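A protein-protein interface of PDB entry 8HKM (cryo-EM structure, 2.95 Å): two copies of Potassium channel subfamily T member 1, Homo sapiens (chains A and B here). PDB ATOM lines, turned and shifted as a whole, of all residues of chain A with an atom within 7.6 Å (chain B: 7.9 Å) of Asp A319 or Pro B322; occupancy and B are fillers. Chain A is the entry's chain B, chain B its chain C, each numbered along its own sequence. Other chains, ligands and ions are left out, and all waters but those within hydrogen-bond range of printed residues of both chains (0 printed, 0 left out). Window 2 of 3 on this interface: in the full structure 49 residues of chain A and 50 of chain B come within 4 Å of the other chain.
Hydrophobic or aromatic side chains of chain B that line the printed part of chain A: Phe B307, Pro B322 and Val B332. Along chain B the printed residues that touch a printed residue of chain A span positions 307 to 332. Of the 13 printed residues of chain A, 4 touch a printed residue of chain B. Printed residues of chain A that touch a printed residue of chain B: Tyr A306, Gly A316, Tyr A317 and Asp A319. Hydrophobic or aromatic side chains of chain A that line the printed part of chain B: Tyr A306 and Tyr A317.
Gly A316 touches its own counterpart, Gly B316. Tyr A317 touches Phe B307, but with the chains exchanged Phe A307 does not touch Tyr B317 (12.5 Å). Tyr A317 touches Gly B316, but with the chains exchanged Gly A316 does not touch Tyr B317 (5.2 Å). Tyr A317 touches its own counterpart, Tyr B317. Positions printed for both chains: 297, 299, 307, 316, 317, 318, 319, 320, 321 and 323. Of the 11 pairs that touch across the chains among the printed residues, 2 have their exchanged pair printed and touching as well.
The side-chain hydroxyl (OH) of Tyr A306 sits at hydrogen-bond distance from the side-chain carboxylate (OD2) of Asp A319, 3.0 Å away. O of Val A310 is in hydrogen-bond range of N of Gly A316, 2.9 Å away. O of Phe B307 lies within hydrogen-bond range of OG1 of Thr B311, at 2.9 Å.
The side-chain hydroxyl (OG1) of Thr B321 sits at hydrogen-bond distance from the side-chain carboxylate (OD2) of Asp A319 (3.3 Å). OG1 of Thr B311 sits close to OH of Tyr A317, at 2.3 Å. The backbone carbonyl oxygen (O) of Tyr A317 sits close to the backbone carbonyl oxygen (O) of Tyr B317, 3.4 Å away.
Among the printed residues, pairs that only touch across the chains: Tyr A317 with Phe B307 (3.2 Å), Tyr A306 with Gln B328 (3.3 Å), Tyr A317 with Gly B318 (3.3 Å), Tyr A306 with Pro B322 (3.4 Å), Gly A316 with Gly B316 (3.6 Å), Tyr A317 with Gly B316 (3.6 Å), Asp A319 with Pro B322 (3.7 Å) and Tyr A306 with Val B332 (3.8 Å).
Printed residues of chain A within 4 Å of Phe B307: Tyr A317. Of the printed residues of chain A, Gly B318 touches Tyr A317. Of the printed residues of chain A, Thr B321 touches Asp A319. Printed residues of chain A within 4 Å of Val B332: Tyr A306 (3.8 Å). The nearest residue of chain B that does not touch Asp A319 is Gln B328 (4.7 Å).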
ATOM      1  N   GLU A 297      28.334   7.769  29.008  1.00  0.00           N
ATOM      2  CA  GLU A 297      27.376   7.443  27.950  1.00  0.00           C
ATOM      3  C   GLU A 297      28.009   7.449  26.562  1.00  0.00           C
ATOM      4  O   GLU A 297      27.371   7.020  25.595  1.00  0.00           O
ATOM      5  CB  GLU A 297      26.172   8.395  27.983  1.00  0.00           C
ATOM      6  CG  GLU A 297      24.853   7.810  27.472  1.00  0.00           C
ATOM      7  CD  GLU A 297      24.397   6.567  28.220  1.00  0.00           C
ATOM      8  OE1 GLU A 297      23.562   5.821  27.665  1.00  0.00           O
ATOM      9  OE2 GLU A 297      24.845   6.345  29.364  1.00  0.00           O
ATOM     10  N   LEU A 299      28.637   9.464  24.081  1.00  0.00           N
ATOM     11  CA  LEU A 299      27.724   9.921  23.042  1.00  0.00           C
ATOM     12  C   LEU A 299      28.451  10.094  21.714  1.00  0.00           C
ATOM     13  O   LEU A 299      29.537  10.679  21.658  1.00  0.00           O
ATOM     14  CB  LEU A 299      27.069  11.238  23.456  1.00  0.00           C
ATOM     15  CG  LEU A 299      26.078  11.160  24.618  1.00  0.00           C
ATOM     16  CD1 LEU A 299      25.575  12.547  24.988  1.00  0.00           C
ATOM     17  CD2 LEU A 299      24.923  10.234  24.273  1.00  0.00           C
ATOM     18  N   THR A 303      24.582  11.919  17.603  1.00  0.00           N
ATOM     19  CA  THR A 303      23.631  11.903  18.710  1.00  0.00           C
ATOM     20  C   THR A 303      23.745  13.168  19.550  1.00  0.00           C
ATOM     21  O   THR A 303      22.732  13.738  19.972  1.00  0.00           O
ATOM     22  CB  THR A 303      23.852  10.661  19.575  1.00  0.00           C
ATOM     23  OG1 THR A 303      23.654   9.484  18.782  1.00  0.00           O
ATOM     24  CG2 THR A 303      22.880  10.643  20.745  1.00  0.00           C
ATOM     25  N   TYR A 306      22.082  16.018  17.644  1.00  0.00           N
ATOM     26  CA  TYR A 306      20.632  15.986  17.800  1.00  0.00           C
ATOM     27  C   TYR A 306      20.222  16.428  19.200  1.00  0.00           C
ATOM     28  O   TYR A 306      19.145  17.007  19.388  1.00  0.00           O
ATOM     29  CB  TYR A 306      20.110  14.581  17.494  1.00  0.00           C
ATOM     30  CG  TYR A 306      18.828  14.210  18.207  1.00  0.00           C
ATOM     31  CD1 TYR A 306      17.602  14.678  17.758  1.00  0.00           C
ATOM     32  CD2 TYR A 306      18.846  13.380  19.321  1.00  0.00           C
ATOM     33  CE1 TYR A 306      16.428  14.338  18.405  1.00  0.00           C
ATOM     34  CE2 TYR A 306      17.677  13.035  19.972  1.00  0.00           C
ATOM     35  CZ  TYR A 306      16.472  13.517  19.510  1.00  0.00           C
ATOM     36  OH  TYR A 306      15.307  13.175  20.156  1.00  0.00           O
ATOM     37  N   PHE A 307      21.070  16.161  20.196  1.00  0.00           N
ATOM     38  CA  PHE A 307      20.769  16.570  21.565  1.00  0.00           C
ATOM     39  C   PHE A 307      20.774  18.088  21.705  1.00  0.00           C
ATOM     40  O   PHE A 307      19.890  18.667  22.347  1.00  0.00           O
ATOM     41  CB  PHE A 307      21.774  15.937  22.528  1.00  0.00           C
ATOM     42  CG  PHE A 307      21.875  16.642  23.850  1.00  0.00           C
ATOM     43  CD1 PHE A 307      20.919  16.445  24.830  1.00  0.00           C
ATOM     44  CD2 PHE A 307      22.929  17.500  24.113  1.00  0.00           C
ATOM     45  CE1 PHE A 307      21.010  17.091  26.046  1.00  0.00           C
ATOM     46  CE2 PHE A 307      23.025  18.150  25.327  1.00  0.00           C
ATOM     47  CZ  PHE A 307      22.065  17.945  26.295  1.00  0.00           C
ATOM     48  N   VAL A 310      17.656  20.028  19.903  1.00  0.00           N
ATOM     49  CA  VAL A 310      16.420  19.984  20.676  1.00  0.00           C
ATOM     50  C   VAL A 310      16.562  20.655  22.031  1.00  0.00           C
ATOM     51  O   VAL A 310      15.550  20.913  22.693  1.00  0.00           O
ATOM     52  CB  VAL A 310      15.940  18.530  20.861  1.00  0.00           C
ATOM     53  CG1 VAL A 310      15.816  17.838  19.512  1.00  0.00           C
ATOM     54  CG2 VAL A 310      16.880  17.766  21.776  1.00  0.00           C
ATOM     55  N   GLY A 316      13.700  19.628  24.549  1.00  0.00           N
ATOM     56  CA  GLY A 316      14.138  18.812  25.666  1.00  0.00           C
ATOM     57  C   GLY A 316      13.583  17.419  25.872  1.00  0.00           C
ATOM     58  O   GLY A 316      13.103  17.095  26.962  1.00  0.00           O
ATOM     59  N   TYR A 317      13.637  16.586  24.830  1.00  0.00           N
ATOM     60  CA  TYR A 317      12.933  15.306  24.830  1.00  0.00           C
ATOM     61  C   TYR A 317      13.243  14.500  26.085  1.00  0.00           C
ATOM     62  O   TYR A 317      12.334  14.011  26.764  1.00  0.00           O
ATOM     63  CB  TYR A 317      13.306  14.507  23.581  1.00  0.00           C
ATOM     64  CG  TYR A 317      12.561  14.933  22.340  1.00  0.00           C
ATOM     65  CD1 TYR A 317      11.200  14.703  22.212  1.00  0.00           C
ATOM     66  CD2 TYR A 317      13.221  15.557  21.292  1.00  0.00           C
ATOM     67  CE1 TYR A 317      10.515  15.089  21.078  1.00  0.00           C
ATOM     68  CE2 TYR A 317      12.547  15.946  20.155  1.00  0.00           C
ATOM     69  CZ  TYR A 317      11.194  15.708  20.052  1.00  0.00           C
ATOM     70  OH  TYR A 317      10.519  16.094  18.919  1.00  0.00           O
ATOM     71  N   GLY A 318      14.523  14.354  26.407  1.00  0.00           N
ATOM     72  CA  GLY A 318      14.941  13.561  27.541  1.00  0.00           C
ATOM     73  C   GLY A 318      15.389  12.152  27.220  1.00  0.00           C
ATOM     74  O   GLY A 318      15.672  11.389  28.150  1.00  0.00           O
ATOM     75  N   ASP A 319      15.455  11.779  25.940  1.00  0.00           N
ATOM     76  CA  ASP A 319      15.972  10.462  25.587  1.00  0.00           C
ATOM     77  C   ASP A 319      17.489  10.406  25.706  1.00  0.00           C
ATOM     78  O   ASP A 319      18.042   9.365  26.080  1.00  0.00           O
ATOM     79  CB  ASP A 319      15.522  10.082  24.176  1.00  0.00           C
ATOM     80  CG  ASP A 319      15.944  11.099  23.132  1.00  0.00           C
ATOM     81  OD1 ASP A 319      16.496  12.154  23.508  1.00  0.00           O
ATOM     82  OD2 ASP A 319      15.723  10.841  21.930  1.00  0.00           O
ATOM     83  N   VAL A 320      18.172  11.504  25.397  1.00  0.00           N
ATOM     84  CA  VAL A 320      19.608  11.641  25.611  1.00  0.00           C
ATOM     85  C   VAL A 320      19.827  12.845  26.517  1.00  0.00           C
ATOM     86  O   VAL A 320      19.541  13.985  26.131  1.00  0.00           O
ATOM     87  CB  VAL A 320      20.378  11.778  24.286  1.00  0.00           C
ATOM     88  CG1 VAL A 320      19.713  12.791  23.357  1.00  0.00           C
ATOM     89  CG2 VAL A 320      21.820  12.174  24.557  1.00  0.00           C
ATOM     90  N   THR A 321      20.309  12.590  27.726  1.00  0.00           N
ATOM     91  CA  THR A 321      20.516  13.608  28.742  1.00  0.00           C
ATOM     92  C   THR A 321      21.897  13.441  29.352  1.00  0.00           C
ATOM     93  O   THR A 321      22.476  12.350  29.311  1.00  0.00           O
ATOM     94  CB  THR A 321      19.460  13.526  29.857  1.00  0.00           C
ATOM     95  OG1 THR A 321      19.850  12.535  30.816  1.00  0.00           O
ATOM     96  CG2 THR A 321      18.092  13.172  29.298  1.00  0.00           C
ATOM     97  N   LYS A 323      24.460  12.654  32.234  1.00  0.00           N
ATOM     98  CA  LYS A 323      24.377  11.723  33.351  1.00  0.00           C
ATOM     99  C   LYS A 323      25.452  11.949  34.402  1.00  0.00           C
ATOM    100  O   LYS A 323      25.436  11.273  35.437  1.00  0.00           O
ATOM    101  CB  LYS A 323      24.445  10.276  32.843  1.00  0.00           C
ATOM    102  CG  LYS A 323      23.166   9.803  32.168  1.00  0.00           C
ATOM    103  CD  LYS A 323      23.326   8.409  31.583  1.00  0.00           C
ATOM    104  CE  LYS A 323      22.008   7.891  31.029  1.00  0.00           C
ATOM    105  NZ  LYS A 323      21.283   8.932  30.250  1.00  0.00           N
ATOM    106  N   PHE B 155      13.109  -4.676  14.414  1.00  0.00           N
ATOM    107  CA  PHE B 155      14.030  -3.707  14.992  1.00  0.00           C
ATOM    108  C   PHE B 155      14.770  -4.345  16.161  1.00  0.00           C
ATOM    109  O   PHE B 155      14.143  -4.858  17.093  1.00  0.00           O
ATOM    110  CB  PHE B 155      13.278  -2.459  15.464  1.00  0.00           C
ATOM    111  CG  PHE B 155      14.170  -1.327  15.916  1.00  0.00           C
ATOM    112  CD1 PHE B 155      13.632  -0.233  16.572  1.00  0.00           C
ATOM    113  CD2 PHE B 155      15.531  -1.332  15.645  1.00  0.00           C
ATOM    114  CE1 PHE B 155      14.436   0.813  16.983  1.00  0.00           C
ATOM    115  CE2 PHE B 155      16.339  -0.289  16.054  1.00  0.00           C
ATOM    116  CZ  PHE B 155      15.791   0.786  16.721  1.00  0.00           C
ATOM    117  N   ILE B 289       8.084  11.751   9.888  1.00  0.00           N
ATOM    118  CA  ILE B 289       8.505  11.045  11.096  1.00  0.00           C
ATOM    119  C   ILE B 289       7.951   9.625  11.110  1.00  0.00           C
ATOM    120  O   ILE B 289       8.610   8.700  11.598  1.00  0.00           O
ATOM    121  CB  ILE B 289       8.101  11.826  12.365  1.00  0.00           C
ATOM    122  CG1 ILE B 289       8.732  11.203  13.609  1.00  0.00           C
ATOM    123  CG2 ILE B 289       6.600  11.849  12.554  1.00  0.00           C
ATOM    124  CD1 ILE B 289      10.201  10.927  13.476  1.00  0.00           C
ATOM    125  N   GLU B 293      10.234   6.241  10.670  1.00  0.00           N
ATOM    126  CA  GLU B 293      10.110   5.314  11.785  1.00  0.00           C
ATOM    127  C   GLU B 293       9.578   3.951  11.365  1.00  0.00           C
ATOM    128  O   GLU B 293       9.325   3.110  12.233  1.00  0.00           O
ATOM    129  CB  GLU B 293       9.203   5.906  12.868  1.00  0.00           C
ATOM    130  N   GLY B 296      12.235   1.754  12.509  1.00  0.00           N
ATOM    131  CA  GLY B 296      12.273   1.574  13.948  1.00  0.00           C
ATOM    132  C   GLY B 296      11.091   2.152  14.698  1.00  0.00           C
ATOM    133  O   GLY B 296      10.700   3.300  14.468  1.00  0.00           O
ATOM    134  N   GLU B 297      10.527   1.349  15.608  1.00  0.00           N
ATOM    135  CA  GLU B 297       9.410   1.690  16.490  1.00  0.00           C
ATOM    136  C   GLU B 297       8.064   1.708  15.773  1.00  0.00           C
ATOM    137  O   GLU B 297       7.021   1.768  16.434  1.00  0.00           O
ATOM    138  CB  GLU B 297       9.644   3.042  17.175  1.00  0.00           C
ATOM    139  CG  GLU B 297      10.518   2.980  18.411  1.00  0.00           C
ATOM    140  CD  GLU B 297      10.074   1.910  19.386  1.00  0.00           C
ATOM    141  OE1 GLU B 297      10.770   0.880  19.497  1.00  0.00           O
ATOM    142  OE2 GLU B 297       9.027   2.099  20.040  1.00  0.00           O
ATOM    143  N   LEU B 299       5.986   3.661  14.218  1.00  0.00           N
ATOM    144  CA  LEU B 299       5.016   4.585  14.795  1.00  0.00           C
ATOM    145  C   LEU B 299       3.758   4.661  13.938  1.00  0.00           C
ATOM    146  O   LEU B 299       3.834   4.763  12.710  1.00  0.00           O
ATOM    147  CB  LEU B 299       5.632   5.975  14.943  1.00  0.00           C
ATOM    148  CG  LEU B 299       6.757   6.123  15.967  1.00  0.00           C
ATOM    149  CD1 LEU B 299       7.313   7.539  15.945  1.00  0.00           C
ATOM    150  CD2 LEU B 299       6.266   5.755  17.357  1.00  0.00           C
ATOM    151  N   PHE B 307       3.179  13.278  18.277  1.00  0.00           N
ATOM    152  CA  PHE B 307       4.592  13.577  18.490  1.00  0.00           C
ATOM    153  C   PHE B 307       4.970  14.925  17.890  1.00  0.00           C
ATOM    154  O   PHE B 307       5.721  15.699  18.493  1.00  0.00           O
ATOM    155  CB  PHE B 307       5.454  12.462  17.894  1.00  0.00           C
ATOM    156  CG  PHE B 307       6.874  12.870  17.630  1.00  0.00           C
ATOM    157  CD1 PHE B 307       7.794  12.924  18.661  1.00  0.00           C
ATOM    158  CD2 PHE B 307       7.287  13.206  16.351  1.00  0.00           C
ATOM    159  CE1 PHE B 307       9.101  13.299  18.423  1.00  0.00           C
ATOM    160  CE2 PHE B 307       8.592  13.586  16.109  1.00  0.00           C
ATOM    161  CZ  PHE B 307       9.501  13.632  17.145  1.00  0.00           C
ATOM    162  N   THR B 311       6.134  18.620  19.556  1.00  0.00           N
ATOM    163  CA  THR B 311       7.494  18.996  19.188  1.00  0.00           C
ATOM    164  C   THR B 311       7.565  20.446  18.724  1.00  0.00           C
ATOM    165  O   THR B 311       8.426  21.205  19.182  1.00  0.00           O
ATOM    166  CB  THR B 311       8.018  18.062  18.095  1.00  0.00           C
ATOM    167  OG1 THR B 311       8.365  16.797  18.671  1.00  0.00           O
ATOM    168  CG2 THR B 311       9.243  18.661  17.418  1.00  0.00           C
ATOM    169  N   GLY B 316       7.866  18.761  24.041  1.00  0.00           N
ATOM    170  CA  GLY B 316       8.833  17.681  24.053  1.00  0.00           C
ATOM    171  C   GLY B 316       8.743  16.659  25.168  1.00  0.00           C
ATOM    172  O   GLY B 316       9.698  16.486  25.931  1.00  0.00           O
ATOM    173  N   TYR B 317       7.560  16.093  25.381  1.00  0.00           N
ATOM    174  CA  TYR B 317       7.390  15.077  26.416  1.00  0.00           C
ATOM    175  C   TYR B 317       8.496  14.035  26.531  1.00  0.00           C
ATOM    176  O   TYR B 317       9.062  13.826  27.609  1.00  0.00           O
ATOM    177  CB  TYR B 317       6.030  14.395  26.271  1.00  0.00           C
ATOM    178  CG  TYR B 317       4.866  15.258  26.690  1.00  0.00           C
ATOM    179  CD1 TYR B 317       4.810  15.813  27.960  1.00  0.00           C
ATOM    180  CD2 TYR B 317       3.819  15.512  25.818  1.00  0.00           C
ATOM    181  CE1 TYR B 317       3.745  16.601  28.347  1.00  0.00           C
ATOM    182  CE2 TYR B 317       2.751  16.297  26.195  1.00  0.00           C
ATOM    183  CZ  TYR B 317       2.719  16.839  27.460  1.00  0.00           C
ATOM    184  OH  TYR B 317       1.654  17.622  27.836  1.00  0.00           O
ATOM    185  N   GLY B 318       8.820  13.375  25.425  1.00  0.00           N
ATOM    186  CA  GLY B 318       9.817  12.328  25.423  1.00  0.00           C
ATOM    187  C   GLY B 318       9.284  10.918  25.536  1.00  0.00           C
ATOM    188  O   GLY B 318      10.085   9.981  25.629  1.00  0.00           O
ATOM    189  N   ASP B 319       7.962  10.734  25.541  1.00  0.00           N
ATOM    190  CA  ASP B 319       7.410   9.384  25.547  1.00  0.00           C
ATOM    191  C   ASP B 319       7.569   8.707  24.193  1.00  0.00           C
ATOM    192  O   ASP B 319       7.811   7.496  24.130  1.00  0.00           O
ATOM    193  CB  ASP B 319       5.940   9.419  25.970  1.00  0.00           C
ATOM    194  CG  ASP B 319       5.096  10.316  25.084  1.00  0.00           C
ATOM    195  OD1 ASP B 319       5.664  10.997  24.204  1.00  0.00           O
ATOM    196  OD2 ASP B 319       3.861  10.342  25.269  1.00  0.00           O
ATOM    197  N   VAL B 320       7.440   9.464  23.106  1.00  0.00           N
ATOM    198  CA  VAL B 320       7.719   8.983  21.758  1.00  0.00           C
ATOM    199  C   VAL B 320       8.811   9.870  21.173  1.00  0.00           C
ATOM    200  O   VAL B 320       8.606  11.075  20.983  1.00  0.00           O
ATOM    201  CB  VAL B 320       6.460   8.978  20.875  1.00  0.00           C
ATOM    202  CG1 VAL B 320       5.654  10.259  21.061  1.00  0.00           C
ATOM    203  CG2 VAL B 320       6.839   8.794  19.413  1.00  0.00           C
ATOM    204  N   THR B 321       9.971   9.283  20.915  1.00  0.00           N
ATOM    205  CA  THR B 321      11.140   9.994  20.423  1.00  0.00           C
ATOM    206  C   THR B 321      11.753   9.231  19.262  1.00  0.00           C
ATOM    207  O   THR B 321      11.548   8.020  19.125  1.00  0.00           O
ATOM    208  CB  THR B 321      12.203  10.178  21.519  1.00  0.00           C
ATOM    209  OG1 THR B 321      13.002   8.992  21.617  1.00  0.00           O
ATOM    210  CG2 THR B 321      11.567  10.469  22.864  1.00  0.00           C
ATOM    211  N   PRO B 322      12.501   9.914  18.397  1.00  0.00           N
ATOM    212  CA  PRO B 322      13.306   9.198  17.404  1.00  0.00           C
ATOM    213  C   PRO B 322      14.328   8.300  18.085  1.00  0.00           C
ATOM    214  O   PRO B 322      14.908   8.656  19.113  1.00  0.00           O
ATOM    215  CB  PRO B 322      13.982  10.327  16.616  1.00  0.00           C
ATOM    216  CG  PRO B 322      13.907  11.525  17.512  1.00  0.00           C
ATOM    217  CD  PRO B 322      12.607  11.374  18.235  1.00  0.00           C
ATOM    218  N   LYS B 323      14.544   7.123  17.501  1.00  0.00           N
ATOM    219  CA  LYS B 323      15.505   6.166  18.029  1.00  0.00           C
ATOM    220  C   LYS B 323      16.561   5.755  17.014  1.00  0.00           C
ATOM    221  O   LYS B 323      17.471   4.994  17.364  1.00  0.00           O
ATOM    222  CB  LYS B 323      14.783   4.919  18.560  1.00  0.00           C
ATOM    223  CG  LYS B 323      14.075   5.141  19.891  1.00  0.00           C
ATOM    224  CD  LYS B 323      13.363   3.884  20.364  1.00  0.00           C
ATOM    225  CE  LYS B 323      12.698   4.097  21.715  1.00  0.00           C
ATOM    226  NZ  LYS B 323      11.996   5.409  21.794  1.00  0.00           N
ATOM    227  N   ILE B 324      16.472   6.232  15.772  1.00  0.00           N
ATOM    228  CA  ILE B 324      17.479   5.973  14.754  1.00  0.00           C
ATOM    229  C   ILE B 324      17.946   7.307  14.188  1.00  0.00           C
ATOM    230  O   ILE B 324      17.219   8.302  14.201  1.00  0.00           O
ATOM    231  CB  ILE B 324      16.958   5.056  13.627  1.00  0.00           C
ATOM    232  CG1 ILE B 324      15.699   5.648  12.990  1.00  0.00           C
ATOM    233  CG2 ILE B 324      16.686   3.659  14.162  1.00  0.00           C
ATOM    234  CD1 ILE B 324      15.139   4.808  11.865  1.00  0.00           C
ATOM    235  N   TRP B 325      19.185   7.317  13.697  1.00  0.00           N
ATOM    236  CA  TRP B 325      19.767   8.563  13.212  1.00  0.00           C
ATOM    237  C   TRP B 325      19.002   9.197  12.047  1.00  0.00           C
ATOM    238  O   TRP B 325      18.899  10.437  12.040  1.00  0.00           O
ATOM    239  CB  TRP B 325      21.259   8.352  12.875  1.00  0.00           C
ATOM    240  CG  TRP B 325      21.572   7.801  11.517  1.00  0.00           C
ATOM    241  CD1 TRP B 325      21.914   6.515  11.215  1.00  0.00           C
ATOM    242  CD2 TRP B 325      21.603   8.526  10.279  1.00  0.00           C
ATOM    243  NE1 TRP B 325      22.135   6.389   9.865  1.00  0.00           N
ATOM    244  CE2 TRP B 325      21.951   7.609   9.268  1.00  0.00           C
ATOM    245  CE3 TRP B 325      21.359   9.856   9.926  1.00  0.00           C
ATOM    246  CZ2 TRP B 325      22.065   7.980   7.931  1.00  0.00           C
ATOM    247  CZ3 TRP B 325      21.469  10.223   8.600  1.00  0.00           C
ATOM    248  CH2 TRP B 325      21.821   9.288   7.618  1.00  0.00           C
ATOM    249  N   PRO B 326      18.473   8.464  11.051  1.00  0.00           N
ATOM    250  CA  PRO B 326      17.665   9.153  10.028  1.00  0.00           C
ATOM    251  C   PRO B 326      16.462   9.867  10.614  1.00  0.00           C
ATOM    252  O   PRO B 326      16.104  10.961  10.162  1.00  0.00           O
ATOM    253  CB  PRO B 326      17.244   8.015   9.090  1.00  0.00           C
ATOM    254  CG  PRO B 326      18.280   6.984   9.263  1.00  0.00           C
ATOM    255  CD  PRO B 326      18.615   7.032  10.726  1.00  0.00           C
ATOM    256  N   SER B 327      15.828   9.268  11.622  1.00  0.00           N
ATOM    257  CA  SER B 327      14.674   9.895  12.253  1.00  0.00           C
ATOM    258  C   SER B 327      15.091  11.081  13.116  1.00  0.00           C
ATOM    259  O   SER B 327      14.371  12.084  13.191  1.00  0.00           O
ATOM    260  CB  SER B 327      13.916   8.863  13.086  1.00  0.00           C
ATOM    261  OG  SER B 327      12.909   9.482  13.861  1.00  0.00           O
ATOM    262  N   GLN B 328      16.237  10.978  13.792  1.00  0.00           N
ATOM    263  CA  GLN B 328      16.735  12.102  14.580  1.00  0.00           C
ATOM    264  C   GLN B 328      17.122  13.273  13.684  1.00  0.00           C
ATOM    265  O   GLN B 328      16.856  14.435  14.012  1.00  0.00           O
ATOM    266  CB  GLN B 328      17.921  11.663  15.442  1.00  0.00           C
ATOM    267  CG  GLN B 328      17.570  10.646  16.515  1.00  0.00           C
ATOM    268  CD  GLN B 328      18.792  10.076  17.207  1.00  0.00           C
ATOM    269  OE1 GLN B 328      19.690   9.536  16.563  1.00  0.00           O
ATOM    270  NE2 GLN B 328      18.831  10.192  18.529  1.00  0.00           N
ATOM    271  N   LEU B 329      17.760  12.983  12.546  1.00  0.00           N
ATOM    272  CA  LEU B 329      18.195  14.044  11.642  1.00  0.00           C
ATOM    273  C   LEU B 329      17.009  14.816  11.077  1.00  0.00           C
ATOM    274  O   LEU B 329      17.069  16.044  10.934  1.00  0.00           O
ATOM    275  CB  LEU B 329      19.042  13.450  10.515  1.00  0.00           C
ATOM    276  CG  LEU B 329      19.500  14.396   9.403  1.00  0.00           C
ATOM    277  CD1 LEU B 329      20.949  14.807   9.608  1.00  0.00           C
ATOM    278  CD2 LEU B 329      19.314  13.743   8.042  1.00  0.00           C
ATOM    279  N   LEU B 330      15.923  14.113  10.744  1.00  0.00           N
ATOM    280  CA  LEU B 330      14.746  14.781  10.198  1.00  0.00           C
ATOM    281  C   LEU B 330      14.152  15.762  11.200  1.00  0.00           C
ATOM    282  O   LEU B 330      13.737  16.866  10.828  1.00  0.00           O
ATOM    283  CB  LEU B 330      13.703  13.747   9.783  1.00  0.00           C
ATOM    284  CG  LEU B 330      12.370  14.301   9.279  1.00  0.00           C
ATOM    285  CD1 LEU B 330      12.480  14.747   7.830  1.00  0.00           C
ATOM    286  CD2 LEU B 330      11.274  13.268   9.450  1.00  0.00           C
ATOM    287  N   VAL B 331      14.099  15.373  12.476  1.00  0.00           N
ATOM    288  CA  VAL B 331      13.567  16.261  13.506  1.00  0.00           C
ATOM    289  C   VAL B 331      14.420  17.517  13.616  1.00  0.00           C
ATOM    290  O   VAL B 331      13.898  18.634  13.729  1.00  0.00           O
ATOM    291  CB  VAL B 331      13.468  15.515  14.850  1.00  0.00           C
ATOM    292  CG1 VAL B 331      13.484  16.490  16.016  1.00  0.00           C
ATOM    293  CG2 VAL B 331      12.216  14.654  14.884  1.00  0.00           C
ATOM    294  N   VAL B 332      15.745  17.358  13.579  1.00  0.00           N
ATOM    295  CA  VAL B 332      16.641  18.509  13.639  1.00  0.00           C
ATOM    296  C   VAL B 332      16.411  19.427  12.445  1.00  0.00           C
ATOM    297  O   VAL B 332      16.305  20.651  12.590  1.00  0.00           O
ATOM    298  CB  VAL B 332      18.106  18.043  13.719  1.00  0.00           C
ATOM    299  CG1 VAL B 332      19.047  19.199  13.425  1.00  0.00           C
ATOM    300  CG2 VAL B 332      18.397  17.439  15.084  1.00  0.00           C
